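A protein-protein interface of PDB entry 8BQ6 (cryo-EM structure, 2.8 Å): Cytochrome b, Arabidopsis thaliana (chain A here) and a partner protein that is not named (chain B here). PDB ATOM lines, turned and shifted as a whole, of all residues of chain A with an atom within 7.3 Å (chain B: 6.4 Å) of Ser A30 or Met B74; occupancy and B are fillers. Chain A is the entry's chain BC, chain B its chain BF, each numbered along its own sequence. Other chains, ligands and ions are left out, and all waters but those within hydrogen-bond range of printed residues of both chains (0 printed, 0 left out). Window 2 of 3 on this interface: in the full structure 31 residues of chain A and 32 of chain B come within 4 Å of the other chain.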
ATOM      1  N   PRO A  27      -5.648 -38.044  20.948  1.00  0.00           N
ATOM      2  CA  PRO A  27      -4.634 -37.249  20.246  1.00  0.00           C
ATOM      3  C   PRO A  27      -4.586 -35.819  20.759  1.00  0.00           C
ATOM      4  O   PRO A  27      -5.614 -35.160  20.925  1.00  0.00           O
ATOM      5  CB  PRO A  27      -5.093 -37.296  18.783  1.00  0.00           C
ATOM      6  CG  PRO A  27      -6.120 -38.388  18.721  1.00  0.00           C
ATOM      7  CD  PRO A  27      -6.758 -38.422  20.063  1.00  0.00           C
ATOM      8  N   THR A  28      -3.365 -35.333  20.977  1.00  0.00           N
ATOM      9  CA  THR A  28      -3.119 -34.026  21.554  1.00  0.00           C
ATOM     10  C   THR A  28      -2.070 -33.312  20.711  1.00  0.00           C
ATOM     11  O   THR A  28      -1.095 -33.944  20.278  1.00  0.00           O
ATOM     12  CB  THR A  28      -2.632 -34.160  23.005  1.00  0.00           C
ATOM     13  OG1 THR A  28      -3.435 -35.131  23.689  1.00  0.00           O
ATOM     14  CG2 THR A  28      -2.738 -32.846  23.732  1.00  0.00           C
ATOM     15  N   PRO A  29      -2.249 -32.018  20.438  1.00  0.00           N
ATOM     16  CA  PRO A  29      -1.219 -31.278  19.696  1.00  0.00           C
ATOM     17  C   PRO A  29       0.124 -31.356  20.401  1.00  0.00           C
ATOM     18  O   PRO A  29       0.227 -31.132  21.608  1.00  0.00           O
ATOM     19  CB  PRO A  29      -1.761 -29.846  19.676  1.00  0.00           C
ATOM     20  CG  PRO A  29      -3.212 -30.012  19.766  1.00  0.00           C
ATOM     21  CD  PRO A  29      -3.436 -31.183  20.680  1.00  0.00           C
ATOM     22  N   SER A  30       1.162 -31.658  19.628  1.00  0.00           N
ATOM     23  CA  SER A  30       2.477 -31.902  20.202  1.00  0.00           C
ATOM     24  C   SER A  30       3.145 -30.636  20.730  1.00  0.00           C
ATOM     25  O   SER A  30       4.132 -30.738  21.462  1.00  0.00           O
ATOM     26  CB  SER A  30       3.369 -32.566  19.159  1.00  0.00           C
ATOM     27  OG  SER A  30       3.661 -31.657  18.114  1.00  0.00           O
ATOM     28  N   ASN A  31       2.632 -29.453  20.392  1.00  0.00           N
ATOM     29  CA  ASN A  31       3.273 -28.198  20.760  1.00  0.00           C
ATOM     30  C   ASN A  31       2.573 -27.488  21.914  1.00  0.00           C
ATOM     31  O   ASN A  31       2.736 -26.274  22.075  1.00  0.00           O
ATOM     32  CB  ASN A  31       3.355 -27.273  19.546  1.00  0.00           C
ATOM     33  CG  ASN A  31       1.997 -26.842  19.058  1.00  0.00           C
ATOM     34  OD1 ASN A  31       1.045 -27.621  19.077  1.00  0.00           O
ATOM     35  ND2 ASN A  31       1.893 -25.595  18.623  1.00  0.00           N
ATOM     36  N   LEU A  32       1.799 -28.216  22.715  1.00  0.00           N
ATOM     37  CA  LEU A  32       1.161 -27.618  23.878  1.00  0.00           C
ATOM     38  C   LEU A  32       2.213 -27.196  24.895  1.00  0.00           C
ATOM     39  O   LEU A  32       3.169 -27.927  25.166  1.00  0.00           O
ATOM     40  CB  LEU A  32       0.189 -28.608  24.520  1.00  0.00           C
ATOM     41  CG  LEU A  32      -1.114 -28.970  23.806  1.00  0.00           C
ATOM     42  CD1 LEU A  32      -2.093 -29.559  24.799  1.00  0.00           C
ATOM     43  CD2 LEU A  32      -1.725 -27.776  23.112  1.00  0.00           C
ATOM     44  N   SER A  33       2.031 -26.011  25.464  1.00  0.00           N
ATOM     45  CA  SER A  33       2.970 -25.484  26.435  1.00  0.00           C
ATOM     46  C   SER A  33       2.514 -25.834  27.850  1.00  0.00           C
ATOM     47  O   SER A  33       1.479 -26.470  28.061  1.00  0.00           O
ATOM     48  CB  SER A  33       3.131 -23.979  26.232  1.00  0.00           C
ATOM     49  OG  SER A  33       2.192 -23.251  26.999  1.00  0.00           O
ATOM     50  N   ASN A 214      -3.931 -25.010  20.312  1.00  0.00           N
ATOM     51  CA  ASN A 214      -2.495 -25.032  20.535  1.00  0.00           C
ATOM     52  C   ASN A 214      -1.952 -23.611  20.519  1.00  0.00           C
ATOM     53  O   ASN A 214      -2.657 -22.677  20.123  1.00  0.00           O
ATOM     54  CB  ASN A 214      -1.791 -25.899  19.478  1.00  0.00           C
ATOM     55  CG  ASN A 214      -1.981 -25.379  18.080  1.00  0.00           C
ATOM     56  OD1 ASN A 214      -1.257 -24.493  17.636  1.00  0.00           O
ATOM     57  ND2 ASN A 214      -2.947 -25.940  17.367  1.00  0.00           N
ATOM     58  N   PRO A 215      -0.715 -23.404  20.988  1.00  0.00           N
ATOM     59  CA  PRO A 215      -0.178 -22.031  21.039  1.00  0.00           C
ATOM     60  C   PRO A 215      -0.150 -21.315  19.701  1.00  0.00           C
ATOM     61  O   PRO A 215      -0.267 -20.083  19.672  1.00  0.00           O
ATOM     62  CB  PRO A 215       1.236 -22.238  21.593  1.00  0.00           C
ATOM     63  CG  PRO A 215       1.113 -23.432  22.441  1.00  0.00           C
ATOM     64  CD  PRO A 215       0.121 -24.338  21.765  1.00  0.00           C
ATOM     65  N   LEU A 216       0.013 -22.034  18.592  1.00  0.00           N
ATOM     66  CA  LEU A 216       0.050 -21.385  17.288  1.00  0.00           C
ATOM     67  C   LEU A 216      -1.336 -21.063  16.749  1.00  0.00           C
ATOM     68  O   LEU A 216      -1.448 -20.276  15.803  1.00  0.00           O
ATOM     69  CB  LEU A 216       0.782 -22.273  16.288  1.00  0.00           C
ATOM     70  CG  LEU A 216       2.297 -22.331  16.431  1.00  0.00           C
ATOM     71  CD1 LEU A 216       2.822 -23.381  15.483  1.00  0.00           C
ATOM     72  CD2 LEU A 216       2.931 -20.978  16.157  1.00  0.00           C
ATOM     73  N   SER A 220      -4.137 -28.689  13.738  1.00  0.00           N
ATOM     74  CA  SER A 220      -3.061 -29.476  14.332  1.00  0.00           C
ATOM     75  C   SER A 220      -3.177 -30.972  14.081  1.00  0.00           C
ATOM     76  O   SER A 220      -2.566 -31.752  14.818  1.00  0.00           O
ATOM     77  CB  SER A 220      -2.992 -29.225  15.840  1.00  0.00           C
ATOM     78  OG  SER A 220      -4.231 -29.509  16.458  1.00  0.00           O
ATOM     79  N   MET A 222      -1.956 -32.788  11.738  1.00  0.00           N
ATOM     80  CA  MET A 222      -0.754 -33.378  11.168  1.00  0.00           C
ATOM     81  C   MET A 222       0.347 -33.635  12.191  1.00  0.00           C
ATOM     82  O   MET A 222       1.306 -34.343  11.869  1.00  0.00           O
ATOM     83  CB  MET A 222      -0.216 -32.485  10.046  1.00  0.00           C
ATOM     84  CG  MET A 222       0.128 -31.071  10.473  1.00  0.00           C
ATOM     85  SD  MET A 222      -1.289 -30.184  11.137  1.00  0.00           S
ATOM     86  CE  MET A 222      -2.205 -29.865   9.636  1.00  0.00           C
ATOM     87  N   ASP A 223       0.250 -33.083  13.399  1.00  0.00           N
ATOM     88  CA  ASP A 223       1.290 -33.269  14.410  1.00  0.00           C
ATOM     89  C   ASP A 223       0.676 -33.538  15.783  1.00  0.00           C
ATOM     90  O   ASP A 223       1.009 -32.889  16.775  1.00  0.00           O
ATOM     91  CB  ASP A 223       2.232 -32.070  14.458  1.00  0.00           C
ATOM     92  CG  ASP A 223       3.531 -32.381  15.179  1.00  0.00           C
ATOM     93  OD1 ASP A 223       3.918 -33.567  15.218  1.00  0.00           O
ATOM     94  OD2 ASP A 223       4.156 -31.445  15.722  1.00  0.00           O
ATOM     95  N   LYS A 224      -0.250 -34.488  15.855  1.00  0.00           N
ATOM     96  CA  LYS A 224      -0.853 -34.885  17.120  1.00  0.00           C
ATOM     97  C   LYS A 224      -0.180 -36.135  17.678  1.00  0.00           C
ATOM     98  O   LYS A 224       0.268 -37.009  16.932  1.00  0.00           O
ATOM     99  CB  LYS A 224      -2.354 -35.129  16.951  1.00  0.00           C
ATOM    100  CG  LYS A 224      -3.203 -33.885  17.155  1.00  0.00           C
ATOM    101  CD  LYS A 224      -4.477 -33.945  16.343  1.00  0.00           C
ATOM    102  CE  LYS A 224      -5.448 -32.863  16.766  1.00  0.00           C
ATOM    103  NZ  LYS A 224      -6.127 -33.211  18.040  1.00  0.00           N
ATOM    104  N   ILE A 225      -0.106 -36.207  19.010  1.00  0.00           N
ATOM    105  CA  ILE A 225       0.453 -37.352  19.721  1.00  0.00           C
ATOM    106  C   ILE A 225      -0.521 -37.761  20.821  1.00  0.00           C
ATOM    107  O   ILE A 225      -1.493 -37.065  21.110  1.00  0.00           O
ATOM    108  CB  ILE A 225       1.846 -37.062  20.320  1.00  0.00           C
ATOM    109  CG1 ILE A 225       1.858 -35.714  21.036  1.00  0.00           C
ATOM    110  CG2 ILE A 225       2.914 -37.079  19.243  1.00  0.00           C
ATOM    111  CD1 ILE A 225       2.927 -35.612  22.088  1.00  0.00           C
ATOM    112  N   PHE A 231       1.882 -36.004  27.627  1.00  0.00           N
ATOM    113  CA  PHE A 231       1.280 -34.971  28.454  1.00  0.00           C
ATOM    114  C   PHE A 231       0.873 -35.485  29.822  1.00  0.00           C
ATOM    115  O   PHE A 231       0.370 -34.706  30.636  1.00  0.00           O
ATOM    116  CB  PHE A 231       0.094 -34.355  27.724  1.00  0.00           C
ATOM    117  CG  PHE A 231       0.492 -33.609  26.498  1.00  0.00           C
ATOM    118  CD1 PHE A 231       1.092 -32.369  26.599  1.00  0.00           C
ATOM    119  CD2 PHE A 231       0.320 -34.166  25.247  1.00  0.00           C
ATOM    120  CE1 PHE A 231       1.481 -31.688  25.479  1.00  0.00           C
ATOM    121  CE2 PHE A 231       0.708 -33.486  24.124  1.00  0.00           C
ATOM    122  CZ  PHE A 231       1.288 -32.246  24.239  1.00  0.00           C
ATOM    123  N   LYS A 234       4.251 -34.382  31.384  1.00  0.00           N
ATOM    124  CA  LYS A 234       4.256 -32.924  31.371  1.00  0.00           C
ATOM    125  C   LYS A 234       3.336 -32.363  32.447  1.00  0.00           C
ATOM    126  O   LYS A 234       3.671 -31.378  33.114  1.00  0.00           O
ATOM    127  CB  LYS A 234       3.833 -32.431  29.994  1.00  0.00           C
ATOM    128  CG  LYS A 234       4.350 -31.075  29.611  1.00  0.00           C
ATOM    129  CD  LYS A 234       4.463 -31.001  28.109  1.00  0.00           C
ATOM    130  CE  LYS A 234       4.715 -29.588  27.629  1.00  0.00           C
ATOM    131  NZ  LYS A 234       5.002 -28.657  28.738  1.00  0.00           N
ATOM    132  N   ALA B  69       5.818 -25.995  11.164  1.00  0.00           N
ATOM    133  CA  ALA B  69       5.620 -24.997  12.211  1.00  0.00           C
ATOM    134  C   ALA B  69       5.349 -25.654  13.556  1.00  0.00           C
ATOM    135  O   ALA B  69       5.845 -25.194  14.591  1.00  0.00           O
ATOM    136  CB  ALA B  69       4.477 -24.057  11.837  1.00  0.00           C
ATOM    137  N   MET B  70       4.551 -26.724  13.561  1.00  0.00           N
ATOM    138  CA  MET B  70       4.273 -27.438  14.801  1.00  0.00           C
ATOM    139  C   MET B  70       5.525 -28.086  15.363  1.00  0.00           C
ATOM    140  O   MET B  70       5.711 -28.143  16.584  1.00  0.00           O
ATOM    141  CB  MET B  70       3.200 -28.493  14.570  1.00  0.00           C
ATOM    142  CG  MET B  70       2.228 -28.605  15.710  1.00  0.00           C
ATOM    143  SD  MET B  70       0.571 -28.963  15.132  1.00  0.00           S
ATOM    144  CE  MET B  70      -0.005 -27.305  14.848  1.00  0.00           C
ATOM    145  N   ASP B  71       6.378 -28.616  14.490  1.00  0.00           N
ATOM    146  CA  ASP B  71       7.619 -29.212  14.964  1.00  0.00           C
ATOM    147  C   ASP B  71       8.541 -28.159  15.565  1.00  0.00           C
ATOM    148  O   ASP B  71       9.188 -28.403  16.588  1.00  0.00           O
ATOM    149  CB  ASP B  71       8.300 -29.965  13.826  1.00  0.00           C
ATOM    150  CG  ASP B  71       9.543 -30.686  14.274  1.00  0.00           C
ATOM    151  OD1 ASP B  71       9.867 -30.618  15.476  1.00  0.00           O
ATOM    152  OD2 ASP B  71      10.184 -31.345  13.429  1.00  0.00           O
ATOM    153  N   LEU B  72       8.622 -26.982  14.941  1.00  0.00           N
ATOM    154  CA  LEU B  72       9.437 -25.915  15.510  1.00  0.00           C
ATOM    155  C   LEU B  72       8.874 -25.450  16.844  1.00  0.00           C
ATOM    156  O   LEU B  72       9.618 -25.287  17.819  1.00  0.00           O
ATOM    157  CB  LEU B  72       9.525 -24.742  14.540  1.00  0.00           C
ATOM    158  CG  LEU B  72      10.341 -24.975  13.276  1.00  0.00           C
ATOM    159  CD1 LEU B  72      10.050 -23.872  12.287  1.00  0.00           C
ATOM    160  CD2 LEU B  72      11.815 -25.029  13.608  1.00  0.00           C
ATOM    161  N   SER B  73       7.558 -25.248  16.907  1.00  0.00           N
ATOM    162  CA  SER B  73       6.931 -24.745  18.124  1.00  0.00           C
ATOM    163  C   SER B  73       7.089 -25.726  19.278  1.00  0.00           C
ATOM    164  O   SER B  73       7.308 -25.319  20.423  1.00  0.00           O
ATOM    165  CB  SER B  73       5.455 -24.452  17.854  1.00  0.00           C
ATOM    166  OG  SER B  73       4.709 -24.392  19.052  1.00  0.00           O
ATOM    167  N   MET B  74       6.970 -27.026  18.997  1.00  0.00           N
ATOM    168  CA  MET B  74       7.205 -28.024  20.035  1.00  0.00           C
ATOM    169  C   MET B  74       8.652 -28.014  20.507  1.00  0.00           C
ATOM    170  O   MET B  74       8.913 -28.160  21.705  1.00  0.00           O
ATOM    171  CB  MET B  74       6.827 -29.413  19.524  1.00  0.00           C
ATOM    172  CG  MET B  74       7.181 -30.535  20.478  1.00  0.00           C
ATOM    173  SD  MET B  74       8.561 -31.521  19.876  1.00  0.00           S
ATOM    174  CE  MET B  74       7.707 -32.737  18.880  1.00  0.00           C
ATOM    175  N   LYS B  75       9.599 -27.839  19.589  1.00  0.00           N
ATOM    176  CA  LYS B  75      11.021 -27.843  19.908  1.00  0.00           C
ATOM    177  C   LYS B  75      11.504 -26.541  20.526  1.00  0.00           C
ATOM    178  O   LYS B  75      12.675 -26.459  20.912  1.00  0.00           O
ATOM    179  CB  LYS B  75      11.845 -28.133  18.652  1.00  0.00           C
ATOM    180  CG  LYS B  75      11.781 -29.566  18.192  1.00  0.00           C
ATOM    181  CD  LYS B  75      12.266 -29.690  16.771  1.00  0.00           C
ATOM    182  CE  LYS B  75      12.833 -31.065  16.520  1.00  0.00           C
ATOM    183  NZ  LYS B  75      13.133 -31.273  15.083  1.00  0.00           N
ATOM    184  N   HIS B  76      10.639 -25.533  20.630  1.00  0.00           N
ATOM    185  CA  HIS B  76      11.024 -24.187  21.053  1.00  0.00           C
ATOM    186  C   HIS B  76      12.121 -23.630  20.145  1.00  0.00           C
ATOM    187  O   HIS B  76      13.085 -23.002  20.589  1.00  0.00           O
ATOM    188  CB  HIS B  76      11.448 -24.168  22.524  1.00  0.00           C
ATOM    189  CG  HIS B  76      11.662 -22.791  23.074  1.00  0.00           C
ATOM    190  ND1 HIS B  76      10.692 -21.813  23.026  1.00  0.00           N
ATOM    191  CD2 HIS B  76      12.728 -22.233  23.692  1.00  0.00           C
ATOM    192  CE1 HIS B  76      11.155 -20.709  23.586  1.00  0.00           C
ATOM    193  NE2 HIS B  76      12.389 -20.937  23.998  1.00  0.00           N
ATOM    194  N   GLU B  77      11.958 -23.861  18.846  1.00  0.00           N
ATOM    195  CA  GLU B  77      12.936 -23.432  17.862  1.00  0.00           C
ATOM    196  C   GLU B  77      12.283 -22.475  16.882  1.00  0.00           C
ATOM    197  O   GLU B  77      11.059 -22.345  16.824  1.00  0.00           O
ATOM    198  CB  GLU B  77      13.514 -24.608  17.079  1.00  0.00           C
ATOM    199  CG  GLU B  77      14.892 -25.009  17.498  1.00  0.00           C
ATOM    200  CD  GLU B  77      15.079 -26.494  17.375  1.00  0.00           C
ATOM    201  OE1 GLU B  77      14.607 -27.072  16.379  1.00  0.00           O
ATOM    202  OE2 GLU B  77      15.640 -27.101  18.297  1.00  0.00           O
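The side-chain hydroxyl (OG) of Ser B73 sits at hydrogen-bond distance from the side-chain amide nitrogen (ND2) of Asn A31 (3.1 Å).
The side-chain carboxylate (OD2) of Asp A223 is in hydrogen-bond range of the side-chain hydroxyl (OG) of Ser A30, 2.5 Å away. The side-chain amide nitrogen of Asn A31 sits at hydrogen-bond distance from the side-chain amide oxygen of Asn A214 (3.5 Å). The side-chain carboxylate (OD1) of Asp B71 lies within salt-bridge range of the side-chain amino group (NZ) of Lys B75, at 3.4 Å. OD1 of Asn A214 sits at hydrogen-bond distance from N of Leu A216.
CG of Met B74 touches O of Ser A30, at 3.2 Å. CG of Met B70 touches OD1 of Asn A31, 3.7 Å away. N of Met B74 touches CB of Asn A31 (3.7 Å). Leu A216 touches Ala B69 (CD1 to O, 3.6 Å). Ser B73 touches Leu A216. Met B70 touches Ser A220. Asp A223 touches Met B70. Asp B71 touches Asp A223.
Of chain B, only Met B74 (3.2 Å) comes within 4 Å of Ser A30. Of chain A, only Ser A30 (3.2 Å) and Asn A31 (3.7 Å) come within 4 Å of Met B74. Printed residues of chain B within 4 Å of Ser A220: Met B70 (3.6 Å). Of the printed residues of chain B, Asp A223 touches Met B70 (3.3 Å) and Asp B71 (3.8 Å). Of the printed residues of chain A, Ala B69 touches Leu A216. Printed residues of chain B within 4 Å of Leu A216: Ala B69 (3.6 Å) and Ser B73 (3.7 Å). Lys B75 touches none of the printed residues of chain A. Leu B72 touches none of the printed residues of chain A.
Of the 9 printed residues of chain B, 5 touch a printed residue of chain A. Of the 17 printed residues of chain A, 5 touch a printed residue of chain B. Among the printed residues, no Asp or Glu carboxylate lies within 4 Å of a Lys or Arg side-chain nitrogen of the other chain.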
